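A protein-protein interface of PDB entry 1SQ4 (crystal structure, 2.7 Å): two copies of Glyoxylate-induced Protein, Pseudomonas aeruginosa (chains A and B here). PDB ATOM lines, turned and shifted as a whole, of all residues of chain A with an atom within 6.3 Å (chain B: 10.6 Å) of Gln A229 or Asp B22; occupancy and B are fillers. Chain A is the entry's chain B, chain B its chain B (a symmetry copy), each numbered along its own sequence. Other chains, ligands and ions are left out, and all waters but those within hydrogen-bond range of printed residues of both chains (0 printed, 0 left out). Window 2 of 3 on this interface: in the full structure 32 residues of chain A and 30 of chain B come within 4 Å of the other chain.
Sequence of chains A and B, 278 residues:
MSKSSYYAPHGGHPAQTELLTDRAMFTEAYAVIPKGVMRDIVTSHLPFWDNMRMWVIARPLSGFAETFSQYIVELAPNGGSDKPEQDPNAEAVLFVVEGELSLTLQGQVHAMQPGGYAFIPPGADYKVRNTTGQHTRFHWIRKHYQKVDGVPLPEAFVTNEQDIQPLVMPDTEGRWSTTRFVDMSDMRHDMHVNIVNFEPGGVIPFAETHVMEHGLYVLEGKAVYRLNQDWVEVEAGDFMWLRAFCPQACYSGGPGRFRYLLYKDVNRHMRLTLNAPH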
ATOM      1  N   PHE A 206      10.756   9.226  -4.974  1.00  0.00           N
ATOM      2  CA  PHE A 206      10.234  10.369  -5.721  1.00  0.00           C
ATOM      3  C   PHE A 206       9.899   9.944  -7.138  1.00  0.00           C
ATOM      4  O   PHE A 206      10.782   9.847  -8.001  1.00  0.00           O
ATOM      5  CB  PHE A 206      11.242  11.516  -5.765  1.00  0.00           C
ATOM      6  CG  PHE A 206      11.764  11.914  -4.417  1.00  0.00           C
ATOM      7  CD1 PHE A 206      12.839  11.238  -3.848  1.00  0.00           C
ATOM      8  CD2 PHE A 206      11.177  12.958  -3.706  1.00  0.00           C
ATOM      9  CE1 PHE A 206      13.329  11.596  -2.597  1.00  0.00           C
ATOM     10  CE2 PHE A 206      11.661  13.322  -2.451  1.00  0.00           C
ATOM     11  CZ  PHE A 206      12.740  12.635  -1.896  1.00  0.00           C
ATOM     12  N   ARG A 226       2.083   5.827  -3.550  1.00  0.00           N
ATOM     13  CA  ARG A 226       2.004   6.760  -2.444  1.00  0.00           C
ATOM     14  C   ARG A 226       1.578   8.141  -2.942  1.00  0.00           C
ATOM     15  O   ARG A 226       2.389   8.912  -3.456  1.00  0.00           O
ATOM     16  CB  ARG A 226       3.369   6.802  -1.749  1.00  0.00           C
ATOM     17  CG  ARG A 226       3.578   7.893  -0.718  1.00  0.00           C
ATOM     18  CD  ARG A 226       2.763   7.676   0.531  1.00  0.00           C
ATOM     19  NE  ARG A 226       3.530   7.971   1.747  1.00  0.00           N
ATOM     20  CZ  ARG A 226       4.075   9.148   2.044  1.00  0.00           C
ATOM     21  NH1 ARG A 226       3.950  10.177   1.215  1.00  0.00           N
ATOM     22  NH2 ARG A 226       4.744   9.299   3.179  1.00  0.00           N
ATOM     23  N   LEU A 227       0.285   8.424  -2.796  1.00  0.00           N
ATOM     24  CA  LEU A 227      -0.321   9.691  -3.203  1.00  0.00           C
ATOM     25  C   LEU A 227      -0.362  10.658  -2.017  1.00  0.00           C
ATOM     26  O   LEU A 227      -1.262  10.590  -1.180  1.00  0.00           O
ATOM     27  CB  LEU A 227      -1.748   9.441  -3.706  1.00  0.00           C
ATOM     28  CG  LEU A 227      -1.854   8.596  -4.974  1.00  0.00           C
ATOM     29  CD1 LEU A 227      -3.290   8.283  -5.285  1.00  0.00           C
ATOM     30  CD2 LEU A 227      -1.213   9.354  -6.120  1.00  0.00           C
ATOM     31  N   ASN A 228       0.615  11.554  -1.947  1.00  0.00           N
ATOM     32  CA  ASN A 228       0.687  12.518  -0.854  1.00  0.00           C
ATOM     33  C   ASN A 228       0.432  11.944   0.542  1.00  0.00           C
ATOM     34  O   ASN A 228      -0.690  12.013   1.042  1.00  0.00           O
ATOM     35  CB  ASN A 228      -0.311  13.649  -1.081  1.00  0.00           C
ATOM     36  CG  ASN A 228      -0.409  14.578   0.111  1.00  0.00           C
ATOM     37  OD1 ASN A 228       0.603  15.117   0.568  1.00  0.00           O
ATOM     38  ND2 ASN A 228      -1.621  14.766   0.627  1.00  0.00           N
ATOM     39  N   GLN A 229       1.457  11.392   1.179  1.00  0.00           N
ATOM     40  CA  GLN A 229       1.300  10.853   2.532  1.00  0.00           C
ATOM     41  C   GLN A 229       0.350   9.641   2.608  1.00  0.00           C
ATOM     42  O   GLN A 229       0.275   8.971   3.641  1.00  0.00           O
ATOM     43  CB  GLN A 229       0.799  11.966   3.480  1.00  0.00           C
ATOM     44  CG  GLN A 229       1.237  11.842   4.950  1.00  0.00           C
ATOM     45  CD  GLN A 229       2.707  12.214   5.167  1.00  0.00           C
ATOM     46  OE1 GLN A 229       3.587  11.815   4.392  1.00  0.00           O
ATOM     47  NE2 GLN A 229       2.979  12.968   6.236  1.00  0.00           N
ATOM     48  N   ASP A 230      -0.368   9.349   1.527  1.00  0.00           N
ATOM     49  CA  ASP A 230      -1.305   8.223   1.526  1.00  0.00           C
ATOM     50  C   ASP A 230      -0.915   7.045   0.609  1.00  0.00           C
ATOM     51  O   ASP A 230      -0.740   7.220  -0.591  1.00  0.00           O
ATOM     52  CB  ASP A 230      -2.710   8.728   1.161  1.00  0.00           C
ATOM     53  CG  ASP A 230      -3.499   9.203   2.374  1.00  0.00           C
ATOM     54  OD1 ASP A 230      -4.524   9.896   2.200  1.00  0.00           O
ATOM     55  OD2 ASP A 230      -3.104   8.868   3.511  1.00  0.00           O
ATOM     56  N   TRP A 231      -0.763   5.850   1.176  1.00  0.00           N
ATOM     57  CA  TRP A 231      -0.429   4.687   0.363  1.00  0.00           C
ATOM     58  C   TRP A 231      -1.716   4.000  -0.086  1.00  0.00           C
ATOM     59  O   TRP A 231      -2.618   3.744   0.719  1.00  0.00           O
ATOM     60  CB  TRP A 231       0.428   3.687   1.133  1.00  0.00           C
ATOM     61  CG  TRP A 231       1.830   4.140   1.383  1.00  0.00           C
ATOM     62  CD1 TRP A 231       2.288   4.813   2.475  1.00  0.00           C
ATOM     63  CD2 TRP A 231       2.969   3.914   0.543  1.00  0.00           C
ATOM     64  NE1 TRP A 231       3.642   5.014   2.373  1.00  0.00           N
ATOM     65  CE2 TRP A 231       4.086   4.477   1.197  1.00  0.00           C
ATOM     66  CE3 TRP A 231       3.154   3.291  -0.697  1.00  0.00           C
ATOM     67  CZ2 TRP A 231       5.371   4.437   0.655  1.00  0.00           C
ATOM     68  CZ3 TRP A 231       4.430   3.245  -1.240  1.00  0.00           C
ATOM     69  CH2 TRP A 231       5.524   3.817  -0.563  1.00  0.00           C
ATOM     70  N   PRO A 247       2.559  14.965  -3.922  1.00  0.00           N
ATOM     71  CA  PRO A 247       3.681  14.031  -3.812  1.00  0.00           C
ATOM     72  C   PRO A 247       3.409  12.681  -4.445  1.00  0.00           C
ATOM     73  O   PRO A 247       2.283  12.193  -4.429  1.00  0.00           O
ATOM     74  CB  PRO A 247       3.894  13.929  -2.303  1.00  0.00           C
ATOM     75  CG  PRO A 247       3.527  15.277  -1.832  1.00  0.00           C
ATOM     76  CD  PRO A 247       2.236  15.518  -2.595  1.00  0.00           C
ATOM     77  N   ASP B  22       6.634  13.484   4.811  1.00  0.00           N
ATOM     78  CA  ASP B  22       6.695  14.673   3.970  1.00  0.00           C
ATOM     79  C   ASP B  22       5.875  15.793   4.591  1.00  0.00           C
ATOM     80  O   ASP B  22       4.925  15.544   5.335  1.00  0.00           O
ATOM     81  CB  ASP B  22       6.165  14.367   2.570  1.00  0.00           C
ATOM     82  CG  ASP B  22       6.544  15.429   1.561  1.00  0.00           C
ATOM     83  OD1 ASP B  22       7.760  15.630   1.352  1.00  0.00           O
ATOM     84  OD2 ASP B  22       5.636  16.062   0.980  1.00  0.00           O
ATOM     85  N   ARG B  23       6.237  17.029   4.260  1.00  0.00           N
ATOM     86  CA  ARG B  23       5.562  18.202   4.804  1.00  0.00           C
ATOM     87  C   ARG B  23       4.618  18.916   3.831  1.00  0.00           C
ATOM     88  O   ARG B  23       4.158  20.022   4.113  1.00  0.00           O
ATOM     89  CB  ARG B  23       6.618  19.180   5.335  1.00  0.00           C
ATOM     90  CG  ARG B  23       7.648  18.493   6.224  1.00  0.00           C
ATOM     91  CD  ARG B  23       8.591  19.451   6.945  1.00  0.00           C
ATOM     92  NE  ARG B  23       9.330  20.326   6.041  1.00  0.00           N
ATOM     93  CZ  ARG B  23       8.886  21.505   5.617  1.00  0.00           C
ATOM     94  NH1 ARG B  23       7.703  21.952   6.013  1.00  0.00           N
ATOM     95  NH2 ARG B  23       9.628  22.244   4.806  1.00  0.00           N
ATOM     96  N   ALA B  24       4.326  18.287   2.695  1.00  0.00           N
ATOM     97  CA  ALA B  24       3.424  18.883   1.711  1.00  0.00           C
ATOM     98  C   ALA B  24       1.998  18.884   2.246  1.00  0.00           C
ATOM     99  O   ALA B  24       1.380  17.830   2.403  1.00  0.00           O
ATOM    100  CB  ALA B  24       3.484  18.112   0.405  1.00  0.00           C
ATOM    101  N   MET B  25       1.479  20.073   2.522  1.00  0.00           N
ATOM    102  CA  MET B  25       0.128  20.204   3.044  1.00  0.00           C
ATOM    103  C   MET B  25      -0.841  20.835   2.051  1.00  0.00           C
ATOM    104  O   MET B  25      -0.467  21.713   1.276  1.00  0.00           O
ATOM    105  CB  MET B  25       0.140  21.023   4.342  1.00  0.00           C
ATOM    106  CG  MET B  25       0.365  20.193   5.599  1.00  0.00           C
ATOM    107  SD  MET B  25      -1.032  18.829   5.834  1.00  0.00           S
ATOM    108  CE  MET B  25      -2.277  19.846   6.916  1.00  0.00           C
ATOM    109  N   PHE B  26      -2.086  20.367   2.081  1.00  0.00           N
ATOM    110  CA  PHE B  26      -3.147  20.874   1.218  1.00  0.00           C
ATOM    111  C   PHE B  26      -4.437  20.918   2.006  1.00  0.00           C
ATOM    112  O   PHE B  26      -5.087  19.893   2.162  1.00  0.00           O
ATOM    113  CB  PHE B  26      -3.336  19.966   0.002  1.00  0.00           C
ATOM    114  CG  PHE B  26      -2.187  19.989  -0.940  1.00  0.00           C
ATOM    115  CD1 PHE B  26      -2.030  21.043  -1.830  1.00  0.00           C
ATOM    116  CD2 PHE B  26      -1.201  19.011  -0.867  1.00  0.00           C
ATOM    117  CE1 PHE B  26      -0.905  21.127  -2.636  1.00  0.00           C
ATOM    118  CE2 PHE B  26      -0.073  19.086  -1.669  1.00  0.00           C
ATOM    119  CZ  PHE B  26       0.082  20.146  -2.550  1.00  0.00           C
ATOM    120  N   VAL B  32       0.980  24.119   1.509  1.00  0.00           N
ATOM    121  CA  VAL B  32       2.399  24.238   1.781  1.00  0.00           C
ATOM    122  C   VAL B  32       3.138  23.267   0.874  1.00  0.00           C
ATOM    123  O   VAL B  32       2.880  22.062   0.908  1.00  0.00           O
ATOM    124  CB  VAL B  32       2.725  23.874   3.239  1.00  0.00           C
ATOM    125  CG1 VAL B  32       4.236  23.945   3.460  1.00  0.00           C
ATOM    126  CG2 VAL B  32       1.999  24.806   4.190  1.00  0.00           C
ATOM    127  N   ILE B  33       4.039  23.790   0.052  1.00  0.00           N
ATOM    128  CA  ILE B  33       4.812  22.926  -0.829  1.00  0.00           C
ATOM    129  C   ILE B  33       6.300  23.059  -0.491  1.00  0.00           C
ATOM    130  O   ILE B  33       6.905  24.106  -0.708  1.00  0.00           O
ATOM    131  CB  ILE B  33       4.581  23.266  -2.335  1.00  0.00           C
ATOM    132  CG1 ILE B  33       5.031  24.693  -2.631  1.00  0.00           C
ATOM    133  CG2 ILE B  33       3.091  23.158  -2.679  1.00  0.00           C
ATOM    134  CD1 ILE B  33       5.410  24.902  -4.087  1.00  0.00           C
ATOM    135  N   PRO B  34       6.898  21.998   0.083  1.00  0.00           N
ATOM    136  CA  PRO B  34       8.316  22.009   0.450  1.00  0.00           C
ATOM    137  C   PRO B  34       9.218  22.136  -0.763  1.00  0.00           C
ATOM    138  O   PRO B  34       8.829  21.819  -1.885  1.00  0.00           O
ATOM    139  CB  PRO B  34       8.505  20.666   1.147  1.00  0.00           C
ATOM    140  CG  PRO B  34       7.177  20.402   1.732  1.00  0.00           C
ATOM    141  CD  PRO B  34       6.239  20.792   0.613  1.00  0.00           C
ATOM    142  N   LYS B  35      10.437  22.588  -0.514  1.00  0.00           N
ATOM    143  CA  LYS B  35      11.416  22.756  -1.562  1.00  0.00           C
ATOM    144  C   LYS B  35      11.817  21.426  -2.206  1.00  0.00           C
ATOM    145  O   LYS B  35      12.201  21.393  -3.377  1.00  0.00           O
ATOM    146  CB  LYS B  35      12.650  23.451  -1.002  1.00  0.00           C
ATOM    147  CG  LYS B  35      13.425  22.633   0.005  1.00  0.00           C
ATOM    148  CD  LYS B  35      14.550  23.481   0.555  1.00  0.00           C
ATOM    149  CE  LYS B  35      15.513  22.723   1.437  1.00  0.00           C
ATOM    150  NZ  LYS B  35      16.435  23.732   2.016  1.00  0.00           N
ATOM    151  N   GLY B  36      11.716  20.335  -1.448  1.00  0.00           N
ATOM    152  CA  GLY B  36      12.079  19.025  -1.962  1.00  0.00           C
ATOM    153  C   GLY B  36      11.392  18.604  -3.249  1.00  0.00           C
ATOM    154  O   GLY B  36      11.667  17.527  -3.780  1.00  0.00           O
ATOM    155  N   VAL B  37      10.507  19.456  -3.758  1.00  0.00           N
ATOM    156  CA  VAL B  37       9.754  19.186  -4.981  1.00  0.00           C
ATOM    157  C   VAL B  37      10.534  19.629  -6.204  1.00  0.00           C
ATOM    158  O   VAL B  37      10.321  19.123  -7.305  1.00  0.00           O
ATOM    159  CB  VAL B  37       8.428  19.951  -4.987  1.00  0.00           C
ATOM    160  CG1 VAL B  37       7.599  19.530  -6.174  1.00  0.00           C
ATOM    161  CG2 VAL B  37       7.685  19.710  -3.693  1.00  0.00           C
ATOM    162  N   MET B  38      11.419  20.598  -5.995  1.00  0.00           N
ATOM    163  CA  MET B  38      12.262  21.157  -7.049  1.00  0.00           C
ATOM    164  C   MET B  38      13.252  20.109  -7.565  1.00  0.00           C
ATOM    165  O   MET B  38      14.442  20.222  -7.292  1.00  0.00           O
ATOM    166  CB  MET B  38      13.073  22.336  -6.497  1.00  0.00           C
ATOM    167  CG  MET B  38      12.316  23.319  -5.619  1.00  0.00           C
ATOM    168  SD  MET B  38      11.257  24.558  -6.635  1.00  0.00           S
ATOM    169  CE  MET B  38       9.794  23.331  -7.062  1.00  0.00           C
ATOM    170  N   ARG B  39      12.780  19.105  -8.308  1.00  0.00           N
ATOM    171  CA  ARG B  39      13.661  18.045  -8.835  1.00  0.00           C
ATOM    172  C   ARG B  39      13.985  18.247 -10.312  1.00  0.00           C
ATOM    173  O   ARG B  39      13.270  18.953 -11.024  1.00  0.00           O
ATOM    174  CB  ARG B  39      13.001  16.678  -8.678  1.00  0.00           C
ATOM    175  CG  ARG B  39      12.313  16.458  -7.344  1.00  0.00           C
ATOM    176  CD  ARG B  39      13.279  15.957  -6.299  1.00  0.00           C
ATOM    177  NE  ARG B  39      13.917  14.726  -6.741  1.00  0.00           N
ATOM    178  CZ  ARG B  39      14.518  13.866  -5.933  1.00  0.00           C
ATOM    179  NH1 ARG B  39      15.082  12.763  -6.430  1.00  0.00           N
ATOM    180  NH2 ARG B  39      14.536  14.101  -4.628  1.00  0.00           N
ATOM    181  N   VAL B 232       3.221  25.054  11.270  1.00  0.00           N
ATOM    182  CA  VAL B 232       4.026  24.256  10.352  1.00  0.00           C
ATOM    183  C   VAL B 232       5.415  24.847  10.172  1.00  0.00           C
ATOM    184  O   VAL B 232       5.565  26.056  10.020  1.00  0.00           O
ATOM    185  CB  VAL B 232       3.362  24.162   8.955  1.00  0.00           C
ATOM    186  CG1 VAL B 232       2.028  23.447   9.049  1.00  0.00           C
ATOM    187  CG2 VAL B 232       3.164  25.554   8.376  1.00  0.00           C
ATOM    188  N   GLU B 233       6.427  23.990  10.197  1.00  0.00           N
ATOM    189  CA  GLU B 233       7.795  24.438  10.007  1.00  0.00           C
ATOM    190  C   GLU B 233       8.054  24.733   8.535  1.00  0.00           C
ATOM    191  O   GLU B 233       7.592  24.006   7.652  1.00  0.00           O
ATOM    192  CB  GLU B 233       8.798  23.379  10.471  1.00  0.00           C
ATOM    193  CG  GLU B 233       9.049  23.340  11.964  1.00  0.00           C
ATOM    194  CD  GLU B 233      10.244  22.476  12.330  1.00  0.00           C
ATOM    195  OE1 GLU B 233      10.140  21.225  12.234  1.00  0.00           O
ATOM    196  OE2 GLU B 233      11.296  23.052  12.710  1.00  0.00           O
ATOM    197  N   GLU B 235      11.191  26.595   5.741  1.00  0.00           N
ATOM    198  CA  GLU B 235      12.563  27.074   5.599  1.00  0.00           C
ATOM    199  C   GLU B 235      12.781  27.624   4.193  1.00  0.00           C
ATOM    200  O   GLU B 235      11.921  27.495   3.320  1.00  0.00           O
ATOM    201  CB  GLU B 235      13.567  25.945   5.895  1.00  0.00           C
ATOM    202  CG  GLU B 235      13.482  24.744   4.960  1.00  0.00           C
ATOM    203  CD  GLU B 235      14.230  23.503   5.469  1.00  0.00           C
ATOM    204  OE1 GLU B 235      14.163  22.460   4.781  1.00  0.00           O
ATOM    205  OE2 GLU B 235      14.877  23.555   6.542  1.00  0.00           O
ATOM    206  N   ASP B 238      10.783  26.810   0.798  1.00  0.00           N
ATOM    207  CA  ASP B 238       9.418  26.368   0.889  1.00  0.00           C
ATOM    208  C   ASP B 238       8.501  27.473   0.371  1.00  0.00           C
ATOM    209  O   ASP B 238       8.868  28.655   0.357  1.00  0.00           O
ATOM    210  CB  ASP B 238       9.070  25.996   2.329  1.00  0.00           C
ATOM    211  CG  ASP B 238       9.951  24.881   2.876  1.00  0.00           C
ATOM    212  OD1 ASP B 238      10.458  24.060   2.074  1.00  0.00           O
ATOM    213  OD2 ASP B 238      10.120  24.819   4.114  1.00  0.00           O
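Arg B39 touches Phe A206.
Pro A247 touches Asp B22.
Ala B24 touches Pro A247 (CB to CG, 3.6 Å).
NE2 of Gln A229 lies within hydrogen-bond range of O of Asp B22 (3.4 Å).
The side-chain amide oxygen of Asn A228 sits close to the backbone carbonyl oxygen of Ala B24 (3.4 Å).
No position is printed for both chains.
Of the 5 pairs that touch across the chains among the printed residues, none has its exchanged pair printed and touching as well.
N of Asn A228 sits at hydrogen-bond distance from O of Pro A247, at 3.1 Å.
The side-chain carboxylate of Asp B22 sits close to the backbone NH of Ala B24 (3.1 Å).
The guanidinium group of Arg A226 sits at hydrogen-bond distance from the side-chain amide oxygen of Gln A229 (3.0 Å).
Gln A229 touches just one residue of chain B: Asp B22 (3.4 Å).
Asp B22 touches just these residues of chain A: Gln A229 (3.4 Å) and Pro A247 (3.6 Å).
Asn A228 touches just one residue of chain B: Ala B24 (3.4 Å).
Pro A247 touches just these residues of chain B: Asp B22 (3.6 Å) and Ala B24 (3.6 Å).
Of the printed residues of chain A, Arg B39 touches Phe A206 (3.4 Å).
Of the printed residues of chain B, Phe A206 touches Arg B39 (3.4 Å).
Printed residues of chain A within 4 Å of Ala B24: Asn A228 (3.4 Å) and Pro A247 (3.6 Å).
The nearest printed residue of chain A that does not touch Ala B24 is Gln A229 (6.0 Å).
Printed residues of chain A that touch a printed residue of chain B: Phe A206, Asn A228, Gln A229 and Pro A247.
Hydrophobic or aromatic side chains of chain A that line the printed part of chain B: Phe A206 and Pro A247.
Of the 17 printed residues of chain B, 3 touch a printed residue of chain A.
Hydrophobic or aromatic side chains of chain B that line the printed part of chain A: Ala B24.
Among the printed residues, 5 pairs touch across the chains.
Among the printed residues, no Asp or Glu carboxylate lies within 4 Å of a Lys or Arg side-chain nitrogen of the other chain.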
